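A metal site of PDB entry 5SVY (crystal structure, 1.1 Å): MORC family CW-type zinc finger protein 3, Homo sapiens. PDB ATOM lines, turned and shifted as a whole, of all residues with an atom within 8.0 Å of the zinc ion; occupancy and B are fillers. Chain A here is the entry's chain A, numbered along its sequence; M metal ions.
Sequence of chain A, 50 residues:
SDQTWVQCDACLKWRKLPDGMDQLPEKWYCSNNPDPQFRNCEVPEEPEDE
The zinc ion is bound by SG of Cys 11, at 2.3 Å. The zinc ion is bound by SG of Cys 41, 2.3 Å away. The side-chain sulfur (SG) of Cys 30 is bound to the zinc ion. SG of Cys 8 is bound to the zinc ion, at 2.4 Å.
SG of Cys 30 sits close to NE of Arg 15 (3.3 Å). NZ of Lys 13 is in hydrogen-bond range of O of Cys 41. SG of Cys 11 sits close to N of Lys 13 (3.5 Å). The side-chain sulfur (SG) of Cys 8 sits close to the backbone NH (N) of Ala 10. N of Cys 8 is in hydrogen-bond range of O of Lys 13 (2.9 Å).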
ATOM      1  N   GLN A   7     -16.546 -27.735  28.538  1.00  0.00           N
ATOM      2  CA  GLN A   7     -15.962 -27.078  27.381  1.00  0.00           C
ATOM      3  C   GLN A   7     -16.865 -27.245  26.174  1.00  0.00           C
ATOM      4  O   GLN A   7     -17.312 -28.349  25.861  1.00  0.00           O
ATOM      5  CB  GLN A   7     -14.569 -27.639  27.077  1.00  0.00           C
ATOM      6  CG  GLN A   7     -13.886 -26.875  25.957  1.00  0.00           C
ATOM      7  CD  GLN A   7     -12.474 -27.299  25.744  1.00  0.00           C
ATOM      8  OE1 GLN A   7     -12.207 -28.494  25.544  1.00  0.00           O
ATOM      9  NE2 GLN A   7     -11.555 -26.352  25.746  1.00  0.00           N
ATOM     10  N   CYS A   8     -17.129 -26.148  25.488  1.00  0.00           N
ATOM     11  CA  CYS A   8     -17.827 -26.202  24.208  1.00  0.00           C
ATOM     12  C   CYS A   8     -16.938 -26.848  23.137  1.00  0.00           C
ATOM     13  O   CYS A   8     -15.817 -26.396  22.902  1.00  0.00           O
ATOM     14  CB  CYS A   8     -18.185 -24.786  23.774  1.00  0.00           C
ATOM     15  SG  CYS A   8     -19.011 -24.742  22.148  1.00  0.00           S
ATOM     16  N   ASP A   9     -17.451 -27.862  22.485  1.00  0.00           N
ATOM     17  CA  ASP A   9     -16.669 -28.550  21.462  1.00  0.00           C
ATOM     18  C   ASP A   9     -16.492 -27.761  20.178  1.00  0.00           C
ATOM     19  O   ASP A   9     -15.644 -28.095  19.374  1.00  0.00           O
ATOM     20  CB  ASP A   9     -17.249 -29.931  21.207  1.00  0.00           C
ATOM     21  CG  ASP A   9     -16.950 -30.883  22.328  1.00  0.00           C
ATOM     22  OD1 ASP A   9     -15.768 -30.986  22.713  1.00  0.00           O
ATOM     23  OD2 ASP A   9     -17.894 -31.502  22.859  1.00  0.00           O
ATOM     24  N   ALA A  10     -17.279 -26.693  20.001  1.00  0.00           N
ATOM     25  CA  ALA A  10     -17.116 -25.822  18.842  1.00  0.00           C
ATOM     26  C   ALA A  10     -16.152 -24.684  19.072  1.00  0.00           C
ATOM     27  O   ALA A  10     -15.270 -24.469  18.255  1.00  0.00           O
ATOM     28  CB  ALA A  10     -18.472 -25.273  18.381  1.00  0.00           C
ATOM     29  N   CYS A  11     -16.331 -23.925  20.153  1.00  0.00           N
ATOM     30  CA  CYS A  11     -15.522 -22.739  20.363  1.00  0.00           C
ATOM     31  C   CYS A  11     -14.443 -22.886  21.431  1.00  0.00           C
ATOM     32  O   CYS A  11     -13.610 -21.984  21.589  1.00  0.00           O
ATOM     33  CB  CYS A  11     -16.406 -21.526  20.680  1.00  0.00           C
ATOM     34  SG  CYS A  11     -17.067 -21.479  22.398  1.00  0.00           S
ATOM     35  N   LEU A  12     -14.471 -23.987  22.163  1.00  0.00           N
ATOM     36  CA  LEU A  12     -13.459 -24.333  23.173  1.00  0.00           C
ATOM     37  C   LEU A  12     -13.516 -23.461  24.428  1.00  0.00           C
ATOM     38  O   LEU A  12     -12.662 -23.615  25.310  1.00  0.00           O
ATOM     39  CB  LEU A  12     -12.046 -24.382  22.580  1.00  0.00           C
ATOM     40  CG  LEU A  12     -11.894 -25.360  21.402  1.00  0.00           C
ATOM     41  CD1 LEU A  12     -10.472 -25.352  20.895  1.00  0.00           C
ATOM     42  CD2 LEU A  12     -12.337 -26.756  21.741  1.00  0.00           C
ATOM     43  N   LYS A  13     -14.532 -22.630  24.582  1.00  0.00           N
ATOM     44  CA  LYS A  13     -14.713 -21.925  25.833  1.00  0.00           C
ATOM     45  C   LYS A  13     -15.231 -22.856  26.911  1.00  0.00           C
ATOM     46  O   LYS A  13     -15.999 -23.782  26.660  1.00  0.00           O
ATOM     47  CB  LYS A  13     -15.693 -20.766  25.677  1.00  0.00           C
ATOM     48  CG  LYS A  13     -15.184 -19.640  24.823  1.00  0.00           C
ATOM     49  CD  LYS A  13     -16.214 -18.523  24.711  1.00  0.00           C
ATOM     50  CE  LYS A  13     -15.787 -17.439  23.764  1.00  0.00           C
ATOM     51  NZ  LYS A  13     -15.755 -17.916  22.381  1.00  0.00           N
ATOM     52  N   TRP A  14     -14.844 -22.563  28.147  1.00  0.00           N
ATOM     53  CA  TRP A  14     -15.359 -23.238  29.320  1.00  0.00           C
ATOM     54  C   TRP A  14     -16.555 -22.476  29.865  1.00  0.00           C
ATOM     55  O   TRP A  14     -16.500 -21.257  30.048  1.00  0.00           O
ATOM     56  CB  TRP A  14     -14.262 -23.328  30.385  1.00  0.00           C
ATOM     57  CG  TRP A  14     -13.104 -24.203  29.948  1.00  0.00           C
ATOM     58  CD1 TRP A  14     -11.983 -23.809  29.295  1.00  0.00           C
ATOM     59  CD2 TRP A  14     -13.000 -25.616  30.100  1.00  0.00           C
ATOM     60  NE1 TRP A  14     -11.170 -24.870  29.034  1.00  0.00           N
ATOM     61  CE2 TRP A  14     -11.774 -26.007  29.527  1.00  0.00           C
ATOM     62  CE3 TRP A  14     -13.805 -26.600  30.685  1.00  0.00           C
ATOM     63  CZ2 TRP A  14     -11.335 -27.311  29.533  1.00  0.00           C
ATOM     64  CZ3 TRP A  14     -13.359 -27.892  30.688  1.00  0.00           C
ATOM     65  CH2 TRP A  14     -12.120 -28.235  30.130  1.00  0.00           C
ATOM     66  N   ARG A  15     -17.631 -23.217  30.145  1.00  0.00           N
ATOM     67  CA  ARG A  15     -18.885 -22.659  30.634  1.00  0.00           C
ATOM     68  C   ARG A  15     -19.205 -23.276  31.994  1.00  0.00           C
ATOM     69  O   ARG A  15     -19.181 -24.494  32.160  1.00  0.00           O
ATOM     70  CB  ARG A  15     -20.015 -22.993  29.664  1.00  0.00           C
ATOM     71  CG  ARG A  15     -19.840 -22.440  28.272  1.00  0.00           C
ATOM     72  CD  ARG A  15     -19.579 -20.956  28.279  1.00  0.00           C
ATOM     73  NE  ARG A  15     -19.721 -20.390  26.944  1.00  0.00           N
ATOM     74  CZ  ARG A  15     -19.442 -19.125  26.615  1.00  0.00           C
ATOM     75  NH1 ARG A  15     -18.901 -18.312  27.508  1.00  0.00           N
ATOM     76  NH2 ARG A  15     -19.669 -18.697  25.384  1.00  0.00           N
ATOM     77  N   TRP A  28     -20.714 -31.324  23.624  1.00  0.00           N
ATOM     78  CA  TRP A  28     -21.531 -30.290  24.240  1.00  0.00           C
ATOM     79  C   TRP A  28     -21.164 -28.963  23.601  1.00  0.00           C
ATOM     80  O   TRP A  28     -20.015 -28.730  23.287  1.00  0.00           O
ATOM     81  CB  TRP A  28     -21.270 -30.240  25.759  1.00  0.00           C
ATOM     82  CG  TRP A  28     -22.150 -29.314  26.534  1.00  0.00           C
ATOM     83  CD1 TRP A  28     -23.300 -29.657  27.189  1.00  0.00           C
ATOM     84  CD2 TRP A  28     -21.975 -27.912  26.739  1.00  0.00           C
ATOM     85  NE1 TRP A  28     -23.850 -28.552  27.792  1.00  0.00           N
ATOM     86  CE2 TRP A  28     -23.040 -27.473  27.540  1.00  0.00           C
ATOM     87  CE3 TRP A  28     -21.001 -26.978  26.350  1.00  0.00           C
ATOM     88  CZ2 TRP A  28     -23.187 -26.144  27.945  1.00  0.00           C
ATOM     89  CZ3 TRP A  28     -21.144 -25.662  26.752  1.00  0.00           C
ATOM     90  CH2 TRP A  28     -22.223 -25.254  27.533  1.00  0.00           C
ATOM     91  N   TYR A  29     -22.157 -28.110  23.416  1.00  0.00           N
ATOM     92  CA  TYR A  29     -21.955 -26.813  22.788  1.00  0.00           C
ATOM     93  C   TYR A  29     -22.648 -25.741  23.614  1.00  0.00           C
ATOM     94  O   TYR A  29     -23.638 -26.010  24.312  1.00  0.00           O
ATOM     95  CB  TYR A  29     -22.567 -26.794  21.386  1.00  0.00           C
ATOM     96  CG  TYR A  29     -22.058 -27.915  20.532  1.00  0.00           C
ATOM     97  CD1 TYR A  29     -20.860 -27.788  19.840  1.00  0.00           C
ATOM     98  CD2 TYR A  29     -22.758 -29.109  20.435  1.00  0.00           C
ATOM     99  CE1 TYR A  29     -20.376 -28.793  19.065  1.00  0.00           C
ATOM    100  CE2 TYR A  29     -22.259 -30.156  19.635  1.00  0.00           C
ATOM    101  CZ  TYR A  29     -21.069 -29.975  18.965  1.00  0.00           C
ATOM    102  OH  TYR A  29     -20.577 -30.989  18.177  1.00  0.00           O
ATOM    103  N   CYS A  30     -22.170 -24.496  23.472  1.00  0.00           N
ATOM    104  CA  CYS A  30     -22.775 -23.372  24.167  1.00  0.00           C
ATOM    105  C   CYS A  30     -24.282 -23.326  23.978  1.00  0.00           C
ATOM    106  O   CYS A  30     -25.010 -22.981  24.898  1.00  0.00           O
ATOM    107  CB  CYS A  30     -22.164 -22.047  23.693  1.00  0.00           C
ATOM    108  SG  CYS A  30     -20.395 -21.860  24.103  1.00  0.00           S
ATOM    109  N   SER A  31     -24.760 -23.658  22.773  1.00  0.00           N
ATOM    110  CA  SER A  31     -26.174 -23.626  22.494  1.00  0.00           C
ATOM    111  C   SER A  31     -27.000 -24.498  23.447  1.00  0.00           C
ATOM    112  O   SER A  31     -28.213 -24.296  23.557  1.00  0.00           O
ATOM    113  CB  SER A  31     -26.403 -24.047  21.059  1.00  0.00           C
ATOM    114  OG  SER A  31     -25.807 -25.274  20.820  1.00  0.00           O
ATOM    115  N   PHE A  38     -25.133 -17.500  28.430  1.00  0.00           N
ATOM    116  CA  PHE A  38     -23.902 -18.122  27.938  1.00  0.00           C
ATOM    117  C   PHE A  38     -24.221 -19.203  26.919  1.00  0.00           C
ATOM    118  O   PHE A  38     -23.574 -20.259  26.857  1.00  0.00           O
ATOM    119  CB  PHE A  38     -23.076 -18.677  29.100  1.00  0.00           C
ATOM    120  CG  PHE A  38     -22.597 -17.627  30.068  1.00  0.00           C
ATOM    121  CD1 PHE A  38     -21.491 -16.875  29.769  1.00  0.00           C
ATOM    122  CD2 PHE A  38     -23.258 -17.403  31.255  1.00  0.00           C
ATOM    123  CE1 PHE A  38     -21.067 -15.901  30.637  1.00  0.00           C
ATOM    124  CE2 PHE A  38     -22.829 -16.442  32.119  1.00  0.00           C
ATOM    125  CZ  PHE A  38     -21.731 -15.686  31.819  1.00  0.00           C
ATOM    126  N   ARG A  39     -25.215 -18.917  26.095  1.00  0.00           N
ATOM    127  CA  ARG A  39     -25.765 -19.881  25.165  1.00  0.00           C
ATOM    128  C   ARG A  39     -25.298 -19.688  23.720  1.00  0.00           C
ATOM    129  O   ARG A  39     -25.750 -20.381  22.809  1.00  0.00           O
ATOM    130  CB  ARG A  39     -27.272 -19.839  25.308  1.00  0.00           C
ATOM    131  CG  ARG A  39     -27.983 -21.070  24.891  1.00  0.00           C
ATOM    132  CD  ARG A  39     -29.459 -20.945  25.163  1.00  0.00           C
ATOM    133  NE  ARG A  39     -29.841 -21.319  26.508  1.00  0.00           N
ATOM    134  CZ  ARG A  39     -31.054 -21.129  27.005  1.00  0.00           C
ATOM    135  NH1 ARG A  39     -32.001 -20.499  26.308  1.00  0.00           N
ATOM    136  NH2 ARG A  39     -31.312 -21.527  28.232  1.00  0.00           N
ATOM    137  N   ASN A  40     -24.401 -18.734  23.521  1.00  0.00           N
ATOM    138  CA  ASN A  40     -23.860 -18.399  22.201  1.00  0.00           C
ATOM    139  C   ASN A  40     -22.352 -18.416  22.301  1.00  0.00           C
ATOM    140  O   ASN A  40     -21.804 -17.874  23.257  1.00  0.00           O
ATOM    141  CB  ASN A  40     -24.370 -16.989  21.770  1.00  0.00           C
ATOM    142  CG  ASN A  40     -24.083 -16.681  20.339  1.00  0.00           C
ATOM    143  OD1 ASN A  40     -22.942 -16.605  19.939  1.00  0.00           O
ATOM    144  ND2 ASN A  40     -25.120 -16.511  19.551  1.00  0.00           N
ATOM    145  N   CYS A  41     -21.700 -19.042  21.319  1.00  0.00           N
ATOM    146  CA  CYS A  41     -20.243 -19.127  21.324  1.00  0.00           C
ATOM    147  C   CYS A  41     -19.556 -17.784  21.333  1.00  0.00           C
ATOM    148  O   CYS A  41     -18.391 -17.705  21.726  1.00  0.00           O
ATOM    149  CB  CYS A  41     -19.752 -19.924  20.127  1.00  0.00           C
ATOM    150  SG  CYS A  41     -20.167 -21.705  20.184  1.00  0.00           S
ATOM    151  N   GLU A  42     -20.234 -16.726  20.925  1.00  0.00           N
ATOM    152  CA  GLU A  42     -19.587 -15.416  20.917  1.00  0.00           C
ATOM    153  C   GLU A  42     -19.472 -14.795  22.301  1.00  0.00           C
ATOM    154  O   GLU A  42     -18.691 -13.860  22.468  1.00  0.00           O
ATOM    155  CB  GLU A  42     -20.299 -14.482  19.956  1.00  0.00           C
ATOM    156  CG  GLU A  42     -20.294 -15.018  18.526  1.00  0.00           C
ATOM    157  CD  GLU A  42     -20.466 -13.940  17.495  1.00  0.00           C
ATOM    158  OE1 GLU A  42     -19.549 -13.115  17.325  1.00  0.00           O
ATOM    159  OE2 GLU A  42     -21.500 -13.915  16.814  1.00  0.00           O
ATOM    160  N   VAL A  43     -20.219 -15.279  23.285  1.00  0.00           N
ATOM    161  CA  VAL A  43     -20.156 -14.678  24.618  1.00  0.00           C
ATOM    162  C   VAL A  43     -18.807 -15.020  25.241  1.00  0.00           C
ATOM    163  O   VAL A  43     -18.447 -16.183  25.307  1.00  0.00           O
ATOM    164  CB  VAL A  43     -21.312 -15.178  25.511  1.00  0.00           C
ATOM    165  CG1 VAL A  43     -21.192 -14.610  26.895  1.00  0.00           C
ATOM    166  CG2 VAL A  43     -22.665 -14.800  24.893  1.00  0.00           C
HETATM  167 ZN    ZN M   1     -19.186 -22.389  22.171  1.00  0.00          ZN
